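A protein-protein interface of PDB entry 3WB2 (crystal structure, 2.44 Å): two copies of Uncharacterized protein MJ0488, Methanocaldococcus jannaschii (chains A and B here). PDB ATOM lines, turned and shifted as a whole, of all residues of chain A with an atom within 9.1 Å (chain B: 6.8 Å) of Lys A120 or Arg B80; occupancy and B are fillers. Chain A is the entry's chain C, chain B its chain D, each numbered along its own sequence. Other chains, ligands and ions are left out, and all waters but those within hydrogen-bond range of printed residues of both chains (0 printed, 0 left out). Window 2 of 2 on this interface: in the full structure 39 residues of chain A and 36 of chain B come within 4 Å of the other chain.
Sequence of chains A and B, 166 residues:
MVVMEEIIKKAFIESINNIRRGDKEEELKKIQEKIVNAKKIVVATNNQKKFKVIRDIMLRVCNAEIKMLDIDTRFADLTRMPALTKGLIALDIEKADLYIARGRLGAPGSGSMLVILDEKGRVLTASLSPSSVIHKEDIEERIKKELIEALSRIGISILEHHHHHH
OE2 of Glu A5 lies within salt-bridge range of NZ of Lys A120 (2.8 Å). OE2 of Glu A5 lies within salt-bridge range of NH2 of Arg A122 (2.8 Å). The side-chain carboxylate of Asp A118 sits at hydrogen-bond distance from the backbone NH of Lys A120. NH1 of Arg A122 is in salt-bridge range of OD2 of Asp A118 (2.8 Å). The backbone carbonyl oxygen (O) of Asp B77 sits at hydrogen-bond distance from the guanidinium group (NH2) of Arg B104. The side-chain hydroxyl (OG) of Ser B110 lies within hydrogen-bond range of the backbone NH (N) of Gly B106 (2.7 Å).
Of the printed residues of chain B, Lys A120 touches Arg B80. Arg B80 touches just these residues of chain A: Lys A120 (2.9 Å), Gly A121 (3.8 Å) and Arg A122 (3.8 Å). Of chain A, only Val A123 comes within 4 Å of Gly B106. Printed residues of chain A within 4 Å of Ala B107: Val A123 (3.0 Å). Of the printed residues of chain B, Phe A12 touches Asp B77 (3.7 Å) and Leu B78 (3.5 Å). Asp A118 touches none of the printed residues of chain B. The nearest printed residue of chain B that does not touch Lys A120 is Ala B107 (9.4 Å). The nearest residue of chain A that does not touch Arg B80 is Val A123 (4.9 Å).
No position is printed for both chains. Of the 9 pairs that touch across the chains among the printed residues, none has its exchanged pair printed and touching as well.
Among the printed residues, merely in contact across the chains: Phe A12 with Asp B77 (3.7 Å), Phe A12 with Leu B78 (3.5 Å), Gly A121 with Arg B80 (3.8 Å), Arg A122 with Arg B80 (3.8 Å), Val A123 with Gly B106 (3.9 Å), Val A123 with Ser B110 (3.8 Å) and Leu A124 with Ser B110 (3.3 Å).
The backbone carbonyl oxygen (O) of Lys A120 sits at hydrogen-bond distance from the guanidinium group (NH2) of Arg B80. The backbone carbonyl oxygen of Val A123 lies within hydrogen-bond range of the backbone NH of Ala B107 (3.0 Å).
Printed residues of chain B that touch a printed residue of chain A: Asp B77, Leu B78, Arg B80, Gly B106, Ala B107 and Ser B110. Hydrophobic or aromatic side chains of chain B within 4 Å of the printed part of chain A: Leu B78 and Ala B107. Hydrophobic or aromatic side chains of chain A that line the printed part of chain B: Phe A12. Among the printed residues, 9 pairs touch across the chains. Among the printed residues, no Asp or Glu carboxylate lies within 4 Å of a Lys or Arg side-chain nitrogen of the other chain.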
ATOM      1  N   VAL A   3     -19.424  -4.919  14.486  1.00  0.00           N
ATOM      2  CA  VAL A   3     -19.615  -4.837  15.961  1.00  0.00           C
ATOM      3  C   VAL A   3     -18.315  -4.977  16.819  1.00  0.00           C
ATOM      4  O   VAL A   3     -17.343  -5.606  16.376  1.00  0.00           O
ATOM      5  CB  VAL A   3     -20.767  -5.763  16.469  1.00  0.00           C
ATOM      6  CG1 VAL A   3     -20.249  -7.141  16.884  1.00  0.00           C
ATOM      7  CG2 VAL A   3     -21.495  -5.096  17.625  1.00  0.00           C
ATOM      8  N   MET A   4     -18.305  -4.381  18.025  1.00  0.00           N
ATOM      9  CA  MET A   4     -17.091  -4.306  18.860  1.00  0.00           C
ATOM     10  C   MET A   4     -16.476  -5.681  19.260  1.00  0.00           C
ATOM     11  O   MET A   4     -15.231  -5.837  19.213  1.00  0.00           O
ATOM     12  CB  MET A   4     -17.334  -3.410  20.085  1.00  0.00           C
ATOM     13  CG  MET A   4     -16.111  -3.140  20.975  1.00  0.00           C
ATOM     14  SD  MET A   4     -15.227  -1.569  20.780  1.00  0.00           S
ATOM     15  CE  MET A   4     -13.737  -2.129  19.948  1.00  0.00           C
ATOM     16  N   GLU A   5     -17.355  -6.644  19.616  1.00  0.00           N
ATOM     17  CA  GLU A   5     -17.004  -8.030  19.895  1.00  0.00           C
ATOM     18  C   GLU A   5     -16.071  -8.649  18.849  1.00  0.00           C
ATOM     19  O   GLU A   5     -15.035  -9.179  19.195  1.00  0.00           O
ATOM     20  CB  GLU A   5     -18.276  -8.878  20.054  1.00  0.00           C
ATOM     21  CG  GLU A   5     -18.974  -8.775  21.406  1.00  0.00           C
ATOM     22  CD  GLU A   5     -19.639  -7.426  21.663  1.00  0.00           C
ATOM     23  OE1 GLU A   5     -19.997  -6.704  20.694  1.00  0.00           O
ATOM     24  OE2 GLU A   5     -19.817  -7.079  22.852  1.00  0.00           O
ATOM     25  N   GLU A   6     -16.440  -8.562  17.580  1.00  0.00           N
ATOM     26  CA  GLU A   6     -15.621  -9.024  16.438  1.00  0.00           C
ATOM     27  C   GLU A   6     -14.236  -8.400  16.303  1.00  0.00           C
ATOM     28  O   GLU A   6     -13.273  -9.108  16.008  1.00  0.00           O
ATOM     29  CB  GLU A   6     -16.340  -8.748  15.100  1.00  0.00           C
ATOM     30  CG  GLU A   6     -17.807  -9.104  15.045  1.00  0.00           C
ATOM     31  CD  GLU A   6     -18.024 -10.507  14.570  1.00  0.00           C
ATOM     32  OE1 GLU A   6     -17.610 -11.447  15.296  1.00  0.00           O
ATOM     33  OE2 GLU A   6     -18.611 -10.650  13.464  1.00  0.00           O
ATOM     34  N   ILE A   8     -12.429  -7.095  18.676  1.00  0.00           N
ATOM     35  CA  ILE A   8     -11.597  -7.488  19.787  1.00  0.00           C
ATOM     36  C   ILE A   8     -11.151  -8.953  19.639  1.00  0.00           C
ATOM     37  O   ILE A   8      -9.980  -9.313  19.965  1.00  0.00           O
ATOM     38  CB  ILE A   8     -12.322  -7.205  21.118  1.00  0.00           C
ATOM     39  CG1 ILE A   8     -12.530  -5.702  21.271  1.00  0.00           C
ATOM     40  CG2 ILE A   8     -11.579  -7.836  22.297  1.00  0.00           C
ATOM     41  CD1 ILE A   8     -13.310  -5.347  22.518  1.00  0.00           C
ATOM     42  N   PHE A  12      -7.412 -10.352  19.632  1.00  0.00           N
ATOM     43  CA  PHE A  12      -7.053 -11.375  20.611  1.00  0.00           C
ATOM     44  C   PHE A  12      -6.320 -12.547  19.944  1.00  0.00           C
ATOM     45  O   PHE A  12      -5.346 -13.083  20.487  1.00  0.00           O
ATOM     46  CB  PHE A  12      -8.298 -11.822  21.404  1.00  0.00           C
ATOM     47  CG  PHE A  12      -8.687 -10.919  22.584  1.00  0.00           C
ATOM     48  CD1 PHE A  12      -8.096  -9.675  22.815  1.00  0.00           C
ATOM     49  CD2 PHE A  12      -9.687 -11.338  23.489  1.00  0.00           C
ATOM     50  CE1 PHE A  12      -8.493  -8.886  23.898  1.00  0.00           C
ATOM     51  CE2 PHE A  12     -10.093 -10.531  24.573  1.00  0.00           C
ATOM     52  CZ  PHE A  12      -9.491  -9.311  24.780  1.00  0.00           C
ATOM     53  N   LYS A  34     -18.352   4.786  18.641  1.00  0.00           N
ATOM     54  CA  LYS A  34     -19.038   4.566  19.903  1.00  0.00           C
ATOM     55  C   LYS A  34     -19.239   5.860  20.675  1.00  0.00           C
ATOM     56  O   LYS A  34     -20.232   6.029  21.389  1.00  0.00           O
ATOM     57  CB  LYS A  34     -18.307   3.518  20.753  1.00  0.00           C
ATOM     58  CG  LYS A  34     -18.704   2.075  20.399  1.00  0.00           C
ATOM     59  CD  LYS A  34     -18.629   1.115  21.600  1.00  0.00           C
ATOM     60  CE  LYS A  34     -19.658  -0.022  21.520  1.00  0.00           C
ATOM     61  NZ  LYS A  34     -19.716  -0.878  22.749  1.00  0.00           N
ATOM     62  N   LEU A  84     -11.558   4.438  38.365  1.00  0.00           N
ATOM     63  CA  LEU A  84     -12.086   3.233  37.796  1.00  0.00           C
ATOM     64  C   LEU A  84     -13.384   2.719  38.542  1.00  0.00           C
ATOM     65  O   LEU A  84     -14.444   2.447  37.902  1.00  0.00           O
ATOM     66  CB  LEU A  84     -10.962   2.190  37.807  1.00  0.00           C
ATOM     67  CG  LEU A  84     -10.829   1.286  36.599  1.00  0.00           C
ATOM     68  CD1 LEU A  84     -12.129   0.508  36.317  1.00  0.00           C
ATOM     69  CD2 LEU A  84     -10.406   2.138  35.403  1.00  0.00           C
ATOM     70  N   GLY A  87     -16.592   4.563  37.859  1.00  0.00           N
ATOM     71  CA  GLY A  87     -17.261   4.162  36.606  1.00  0.00           C
ATOM     72  C   GLY A  87     -18.132   2.922  36.711  1.00  0.00           C
ATOM     73  O   GLY A  87     -19.229   2.870  36.139  1.00  0.00           O
ATOM     74  N   LEU A  88     -17.643   1.951  37.473  1.00  0.00           N
ATOM     75  CA  LEU A  88     -18.265   0.676  37.619  1.00  0.00           C
ATOM     76  C   LEU A  88     -19.474   0.778  38.540  1.00  0.00           C
ATOM     77  O   LEU A  88     -20.405  -0.023  38.451  1.00  0.00           O
ATOM     78  CB  LEU A  88     -17.243  -0.315  38.165  1.00  0.00           C
ATOM     79  CG  LEU A  88     -16.117  -0.832  37.221  1.00  0.00           C
ATOM     80  CD1 LEU A  88     -15.132  -1.768  37.907  1.00  0.00           C
ATOM     81  CD2 LEU A  88     -16.611  -1.516  35.961  1.00  0.00           C
ATOM     82  N   LEU A  91     -22.126   2.036  36.236  1.00  0.00           N
ATOM     83  CA  LEU A  91     -22.501   0.965  35.356  1.00  0.00           C
ATOM     84  C   LEU A  91     -23.467   0.018  36.059  1.00  0.00           C
ATOM     85  O   LEU A  91     -24.395  -0.477  35.420  1.00  0.00           O
ATOM     86  CB  LEU A  91     -21.245   0.229  34.821  1.00  0.00           C
ATOM     87  CG  LEU A  91     -21.452  -1.081  34.045  1.00  0.00           C
ATOM     88  CD1 LEU A  91     -21.690  -0.778  32.575  1.00  0.00           C
ATOM     89  CD2 LEU A  91     -20.297  -2.061  34.170  1.00  0.00           C
ATOM     90  N   GLU A  94     -27.289   2.244  36.317  1.00  0.00           N
ATOM     91  CA  GLU A  94     -27.940   2.980  35.219  1.00  0.00           C
ATOM     92  C   GLU A  94     -27.602   2.315  33.915  1.00  0.00           C
ATOM     93  O   GLU A  94     -26.458   1.937  33.715  1.00  0.00           O
ATOM     94  CB  GLU A  94     -27.440   4.430  35.103  1.00  0.00           C
ATOM     95  CG  GLU A  94     -27.934   5.454  36.116  1.00  0.00           C
ATOM     96  CD  GLU A  94     -29.271   6.081  35.749  1.00  0.00           C
ATOM     97  OE1 GLU A  94     -29.771   5.866  34.629  1.00  0.00           O
ATOM     98  OE2 GLU A  94     -29.831   6.798  36.601  1.00  0.00           O
ATOM     99  N   ALA A  96     -26.730   2.836  30.132  1.00  0.00           N
ATOM    100  CA  ALA A  96     -26.214   3.886  29.246  1.00  0.00           C
ATOM    101  C   ALA A  96     -25.211   3.313  28.268  1.00  0.00           C
ATOM    102  O   ALA A  96     -24.740   2.202  28.442  1.00  0.00           O
ATOM    103  CB  ALA A  96     -25.590   5.033  30.036  1.00  0.00           C
ATOM    104  N   ASP A  97     -24.889   4.092  27.240  1.00  0.00           N
ATOM    105  CA  ASP A  97     -23.985   3.679  26.174  1.00  0.00           C
ATOM    106  C   ASP A  97     -22.564   4.083  26.560  1.00  0.00           C
ATOM    107  O   ASP A  97     -21.627   3.483  26.067  1.00  0.00           O
ATOM    108  CB  ASP A  97     -24.390   4.305  24.799  1.00  0.00           C
ATOM    109  CG  ASP A  97     -25.843   3.922  24.351  1.00  0.00           C
ATOM    110  OD1 ASP A  97     -26.154   2.707  24.227  1.00  0.00           O
ATOM    111  OD2 ASP A  97     -26.677   4.841  24.111  1.00  0.00           O
ATOM    112  N   LEU A  98     -22.409   5.062  27.463  1.00  0.00           N
ATOM    113  CA  LEU A  98     -21.100   5.598  27.822  1.00  0.00           C
ATOM    114  C   LEU A  98     -21.081   6.091  29.289  1.00  0.00           C
ATOM    115  O   LEU A  98     -22.046   6.715  29.718  1.00  0.00           O
ATOM    116  CB  LEU A  98     -20.838   6.737  26.859  1.00  0.00           C
ATOM    117  CG  LEU A  98     -19.546   6.934  26.093  1.00  0.00           C
ATOM    118  CD1 LEU A  98     -18.596   7.342  27.183  1.00  0.00           C
ATOM    119  CD2 LEU A  98     -19.044   5.677  25.402  1.00  0.00           C
ATOM    120  N   TYR A  99     -20.043   5.761  30.072  1.00  0.00           N
ATOM    121  CA  TYR A  99     -19.879   6.246  31.478  1.00  0.00           C
ATOM    122  C   TYR A  99     -18.569   7.050  31.588  1.00  0.00           C
ATOM    123  O   TYR A  99     -17.521   6.581  31.140  1.00  0.00           O
ATOM    124  CB  TYR A  99     -19.867   5.086  32.509  1.00  0.00           C
ATOM    125  CG  TYR A  99     -21.068   4.168  32.403  1.00  0.00           C
ATOM    126  CD1 TYR A  99     -21.099   3.119  31.487  1.00  0.00           C
ATOM    127  CD2 TYR A  99     -22.197   4.373  33.197  1.00  0.00           C
ATOM    128  CE1 TYR A  99     -22.218   2.308  31.371  1.00  0.00           C
ATOM    129  CE2 TYR A  99     -23.314   3.574  33.079  1.00  0.00           C
ATOM    130  CZ  TYR A  99     -23.319   2.544  32.167  1.00  0.00           C
ATOM    131  OH  TYR A  99     -24.446   1.752  32.059  1.00  0.00           O
ATOM    132  N   LEU A 117     -15.794   4.747  29.848  1.00  0.00           N
ATOM    133  CA  LEU A 117     -16.106   3.296  29.747  1.00  0.00           C
ATOM    134  C   LEU A 117     -17.252   3.129  28.744  1.00  0.00           C
ATOM    135  O   LEU A 117     -18.070   4.060  28.590  1.00  0.00           O
ATOM    136  CB  LEU A 117     -16.457   2.677  31.129  1.00  0.00           C
ATOM    137  CG  LEU A 117     -15.393   2.796  32.247  1.00  0.00           C
ATOM    138  CD1 LEU A 117     -15.766   2.143  33.572  1.00  0.00           C
ATOM    139  CD2 LEU A 117     -14.071   2.188  31.832  1.00  0.00           C
ATOM    140  N   ASP A 118     -17.310   1.978  28.050  1.00  0.00           N
ATOM    141  CA  ASP A 118     -18.499   1.639  27.214  1.00  0.00           C
ATOM    142  C   ASP A 118     -19.542   0.862  28.031  1.00  0.00           C
ATOM    143  O   ASP A 118     -19.327   0.625  29.221  1.00  0.00           O
ATOM    144  CB  ASP A 118     -18.119   0.923  25.913  1.00  0.00           C
ATOM    145  CG  ASP A 118     -17.734  -0.558  26.118  1.00  0.00           C
ATOM    146  OD1 ASP A 118     -17.769  -1.092  27.269  1.00  0.00           O
ATOM    147  OD2 ASP A 118     -17.410  -1.206  25.091  1.00  0.00           O
ATOM    148  N   GLU A 119     -20.661   0.472  27.407  1.00  0.00           N
ATOM    149  CA  GLU A 119     -21.771  -0.186  28.126  1.00  0.00           C
ATOM    150  C   GLU A 119     -21.436  -1.533  28.762  1.00  0.00           C
ATOM    151  O   GLU A 119     -22.291  -2.129  29.411  1.00  0.00           O
ATOM    152  CB  GLU A 119     -23.007  -0.308  27.212  1.00  0.00           C
ATOM    153  CG  GLU A 119     -23.169  -1.622  26.444  1.00  0.00           C
ATOM    154  CD  GLU A 119     -22.453  -1.657  25.099  1.00  0.00           C
ATOM    155  OE1 GLU A 119     -21.301  -1.150  24.961  1.00  0.00           O
ATOM    156  OE2 GLU A 119     -23.068  -2.214  24.168  1.00  0.00           O
ATOM    157  N   LYS A 120     -20.223  -2.044  28.552  1.00  0.00           N
ATOM    158  CA  LYS A 120     -19.832  -3.326  29.180  1.00  0.00           C
ATOM    159  C   LYS A 120     -18.582  -3.172  30.019  1.00  0.00           C
ATOM    160  O   LYS A 120     -17.947  -4.172  30.436  1.00  0.00           O
ATOM    161  CB  LYS A 120     -19.647  -4.440  28.155  1.00  0.00           C
ATOM    162  CG  LYS A 120     -20.927  -5.007  27.537  1.00  0.00           C
ATOM    163  CD  LYS A 120     -20.457  -6.058  26.551  1.00  0.00           C
ATOM    164  CE  LYS A 120     -21.428  -7.194  26.208  1.00  0.00           C
ATOM    165  NZ  LYS A 120     -20.628  -8.168  25.357  1.00  0.00           N
ATOM    166  N   GLY A 121     -18.219  -1.914  30.268  1.00  0.00           N
ATOM    167  CA  GLY A 121     -17.193  -1.618  31.234  1.00  0.00           C
ATOM    168  C   GLY A 121     -15.812  -1.572  30.663  1.00  0.00           C
ATOM    169  O   GLY A 121     -14.865  -1.380  31.394  1.00  0.00           O
ATOM    170  N   ARG A 122     -15.688  -1.755  29.351  1.00  0.00           N
ATOM    171  CA  ARG A 122     -14.398  -1.656  28.666  1.00  0.00           C
ATOM    172  C   ARG A 122     -13.842  -0.238  28.770  1.00  0.00           C
ATOM    173  O   ARG A 122     -14.605   0.747  28.667  1.00  0.00           O
ATOM    174  CB  ARG A 122     -14.516  -2.062  27.189  1.00  0.00           C
ATOM    175  CG  ARG A 122     -14.955  -3.509  26.988  1.00  0.00           C
ATOM    176  CD  ARG A 122     -15.119  -3.795  25.523  1.00  0.00           C
ATOM    177  NE  ARG A 122     -15.839  -5.013  25.175  1.00  0.00           N
ATOM    178  CZ  ARG A 122     -17.075  -5.038  24.656  1.00  0.00           C
ATOM    179  NH1 ARG A 122     -17.744  -3.905  24.486  1.00  0.00           N
ATOM    180  NH2 ARG A 122     -17.642  -6.194  24.290  1.00  0.00           N
ATOM    181  N   VAL A 123     -12.518  -0.154  28.930  1.00  0.00           N
ATOM    182  CA  VAL A 123     -11.775   1.102  28.975  1.00  0.00           C
ATOM    183  C   VAL A 123     -11.422   1.565  27.560  1.00  0.00           C
ATOM    184  O   VAL A 123     -10.574   0.939  26.892  1.00  0.00           O
ATOM    185  CB  VAL A 123     -10.473   0.920  29.807  1.00  0.00           C
ATOM    186  CG1 VAL A 123      -9.652   2.229  29.887  1.00  0.00           C
ATOM    187  CG2 VAL A 123     -10.836   0.349  31.178  1.00  0.00           C
ATOM    188  N   LEU A 124     -12.064   2.662  27.108  1.00  0.00           N
ATOM    189  CA  LEU A 124     -11.857   3.209  25.754  1.00  0.00           C
ATOM    190  C   LEU A 124     -10.705   4.236  25.642  1.00  0.00           C
ATOM    191  O   LEU A 124      -9.990   4.222  24.640  1.00  0.00           O
ATOM    192  CB  LEU A 124     -13.145   3.840  25.168  1.00  0.00           C
ATOM    193  CG  LEU A 124     -14.430   3.004  25.186  1.00  0.00           C
ATOM    194  CD1 LEU A 124     -15.459   3.773  24.368  1.00  0.00           C
ATOM    195  CD2 LEU A 124     -14.216   1.603  24.619  1.00  0.00           C
ATOM    196  N   ALA B  76      -0.939 -11.516  28.966  1.00  0.00           N
ATOM    197  CA  ALA B  76      -1.415 -10.230  29.466  1.00  0.00           C
ATOM    198  C   ALA B  76      -2.354  -9.462  28.494  1.00  0.00           C
ATOM    199  O   ALA B  76      -3.261  -8.750  28.934  1.00  0.00           O
ATOM    200  CB  ALA B  76      -0.253  -9.357  29.923  1.00  0.00           C
ATOM    201  N   ASP B  77      -2.180  -9.655  27.195  1.00  0.00           N
ATOM    202  CA  ASP B  77      -2.905  -8.834  26.214  1.00  0.00           C
ATOM    203  C   ASP B  77      -4.337  -9.321  25.889  1.00  0.00           C
ATOM    204  O   ASP B  77      -4.985  -8.757  25.005  1.00  0.00           O
ATOM    205  CB  ASP B  77      -2.077  -8.682  24.930  1.00  0.00           C
ATOM    206  CG  ASP B  77      -0.715  -8.005  25.170  1.00  0.00           C
ATOM    207  OD1 ASP B  77      -0.593  -7.193  26.130  1.00  0.00           O
ATOM    208  OD2 ASP B  77       0.243  -8.281  24.379  1.00  0.00           O
ATOM    209  N   LEU B  78      -4.853 -10.343  26.593  1.00  0.00           N
ATOM    210  CA  LEU B  78      -6.288 -10.655  26.479  1.00  0.00           C
ATOM    211  C   LEU B  78      -7.052 -10.201  27.748  1.00  0.00           C
ATOM    212  O   LEU B  78      -8.290 -10.465  27.888  1.00  0.00           O
ATOM    213  CB  LEU B  78      -6.538 -12.131  26.181  1.00  0.00           C
ATOM    214  CG  LEU B  78      -6.296 -12.691  24.772  1.00  0.00           C
ATOM    215  CD1 LEU B  78      -4.821 -12.630  24.465  1.00  0.00           C
ATOM    216  CD2 LEU B  78      -6.774 -14.127  24.638  1.00  0.00           C
ATOM    217  N   THR B  79      -6.343  -9.533  28.671  1.00  0.00           N
ATOM    218  CA  THR B  79      -7.007  -9.012  29.903  1.00  0.00           C
ATOM    219  C   THR B  79      -7.583  -7.612  29.683  1.00  0.00           C
ATOM    220  O   THR B  79      -7.273  -6.974  28.684  1.00  0.00           O
ATOM    221  CB  THR B  79      -6.077  -9.121  31.145  1.00  0.00           C
ATOM    222  OG1 THR B  79      -4.989  -8.199  31.050  1.00  0.00           O
ATOM    223  CG2 THR B  79      -5.513 -10.591  31.282  1.00  0.00           C
ATOM    224  N   ARG B  80      -8.450  -7.140  30.566  1.00  0.00           N
ATOM    225  CA  ARG B  80      -9.042  -5.787  30.440  1.00  0.00           C
ATOM    226  C   ARG B  80      -8.058  -4.605  30.360  1.00  0.00           C
ATOM    227  O   ARG B  80      -8.334  -3.555  29.693  1.00  0.00           O
ATOM    228  CB  ARG B  80     -10.028  -5.517  31.587  1.00  0.00           C
ATOM    229  CG  ARG B  80     -11.465  -5.300  31.096  1.00  0.00           C
ATOM    230  CD  ARG B  80     -12.238  -6.602  30.947  1.00  0.00           C
ATOM    231  NE  ARG B  80     -13.508  -6.505  30.198  1.00  0.00           N
ATOM    232  CZ  ARG B  80     -14.620  -5.864  30.574  1.00  0.00           C
ATOM    233  NH1 ARG B  80     -14.689  -5.145  31.677  1.00  0.00           N
ATOM    234  NH2 ARG B  80     -15.685  -5.909  29.800  1.00  0.00           N
ATOM    235  N   MET B  81      -6.932  -4.765  31.055  1.00  0.00           N
ATOM    236  CA  MET B  81      -5.984  -3.702  31.259  1.00  0.00           C
ATOM    237  C   MET B  81      -4.553  -4.260  31.236  1.00  0.00           C
ATOM    238  O   MET B  81      -3.934  -4.461  32.259  1.00  0.00           O
ATOM    239  CB  MET B  81      -6.290  -2.919  32.551  1.00  0.00           C
ATOM    240  CG  MET B  81      -7.523  -1.978  32.470  1.00  0.00           C
ATOM    241  SD  MET B  81      -7.744  -0.867  33.918  1.00  0.00           S
ATOM    242  CE  MET B  81      -6.634   0.532  33.629  1.00  0.00           C
ATOM    243  N   PRO B  82      -4.021  -4.452  30.028  1.00  0.00           N
ATOM    244  CA  PRO B  82      -2.783  -5.201  29.848  1.00  0.00           C
ATOM    245  C   PRO B  82      -1.538  -4.705  30.623  1.00  0.00           C
ATOM    246  O   PRO B  82      -0.802  -5.570  31.176  1.00  0.00           O
ATOM    247  CB  PRO B  82      -2.600  -5.196  28.338  1.00  0.00           C
ATOM    248  CG  PRO B  82      -4.053  -5.197  27.837  1.00  0.00           C
ATOM    249  CD  PRO B  82      -4.693  -4.171  28.732  1.00  0.00           C
ATOM    250  N   THR B  85      -1.909  -5.562  34.302  1.00  0.00           N
ATOM    251  CA  THR B  85      -1.696  -7.007  34.416  1.00  0.00           C
ATOM    252  C   THR B  85      -0.194  -7.364  34.421  1.00  0.00           C
ATOM    253  O   THR B  85       0.247  -8.168  35.258  1.00  0.00           O
ATOM    254  CB  THR B  85      -2.524  -7.753  33.334  1.00  0.00           C
ATOM    255  OG1 THR B  85      -3.919  -7.554  33.621  1.00  0.00           O
ATOM    256  CG2 THR B  85      -2.260  -9.278  33.331  1.00  0.00           C
ATOM    257  N   ARG B 104      -0.603  -2.076  26.454  1.00  0.00           N
ATOM    258  CA  ARG B 104      -1.874  -1.435  26.118  1.00  0.00           C
ATOM    259  C   ARG B 104      -2.647  -1.023  27.378  1.00  0.00           C
ATOM    260  O   ARG B 104      -2.709  -1.775  28.353  1.00  0.00           O
ATOM    261  CB  ARG B 104      -2.746  -2.316  25.219  1.00  0.00           C
ATOM    262  CG  ARG B 104      -4.002  -1.624  24.725  1.00  0.00           C
ATOM    263  CD  ARG B 104      -4.674  -2.469  23.670  1.00  0.00           C
ATOM    264  NE  ARG B 104      -5.359  -3.604  24.279  1.00  0.00           N
ATOM    265  CZ  ARG B 104      -5.202  -4.883  23.935  1.00  0.00           C
ATOM    266  NH1 ARG B 104      -4.369  -5.269  22.963  1.00  0.00           N
ATOM    267  NH2 ARG B 104      -5.918  -5.785  24.552  1.00  0.00           N
ATOM    268  N   LEU B 105      -3.240   0.174  27.332  1.00  0.00           N
ATOM    269  CA  LEU B 105      -3.988   0.735  28.446  1.00  0.00           C
ATOM    270  C   LEU B 105      -5.243  -0.084  28.804  1.00  0.00           C
ATOM    271  O   LEU B 105      -5.394  -0.539  29.966  1.00  0.00           O
ATOM    272  CB  LEU B 105      -4.358   2.189  28.102  1.00  0.00           C
ATOM    273  CG  LEU B 105      -5.467   2.808  28.960  1.00  0.00           C
ATOM    274  CD1 LEU B 105      -5.023   2.931  30.417  1.00  0.00           C
ATOM    275  CD2 LEU B 105      -5.940   4.159  28.420  1.00  0.00           C
ATOM    276  N   GLY B 106      -6.147  -0.233  27.827  1.00  0.00           N
ATOM    277  CA  GLY B 106      -7.373  -1.006  28.010  1.00  0.00           C
ATOM    278  C   GLY B 106      -7.786  -1.839  26.774  1.00  0.00           C
ATOM    279  O   GLY B 106      -7.078  -2.778  26.353  1.00  0.00           O
ATOM    280  N   ALA B 107      -8.963  -1.516  26.223  1.00  0.00           N
ATOM    281  CA  ALA B 107      -9.510  -2.180  25.050  1.00  0.00           C
ATOM    282  C   ALA B 107      -8.619  -1.895  23.850  1.00  0.00           C
ATOM    283  O   ALA B 107      -7.875  -0.901  23.844  1.00  0.00           O
ATOM    284  CB  ALA B 107     -10.910  -1.713  24.784  1.00  0.00           C
ATOM    285  N   SER B 110      -7.147   1.546  22.465  1.00  0.00           N
ATOM    286  CA  SER B 110      -6.994   2.528  23.557  1.00  0.00           C
ATOM    287  C   SER B 110      -5.599   3.197  23.772  1.00  0.00           C
ATOM    288  O   SER B 110      -5.473   4.082  24.636  1.00  0.00           O
ATOM    289  CB  SER B 110      -7.527   2.001  24.907  1.00  0.00           C
ATOM    290  OG  SER B 110      -6.735   0.940  25.414  1.00  0.00           O
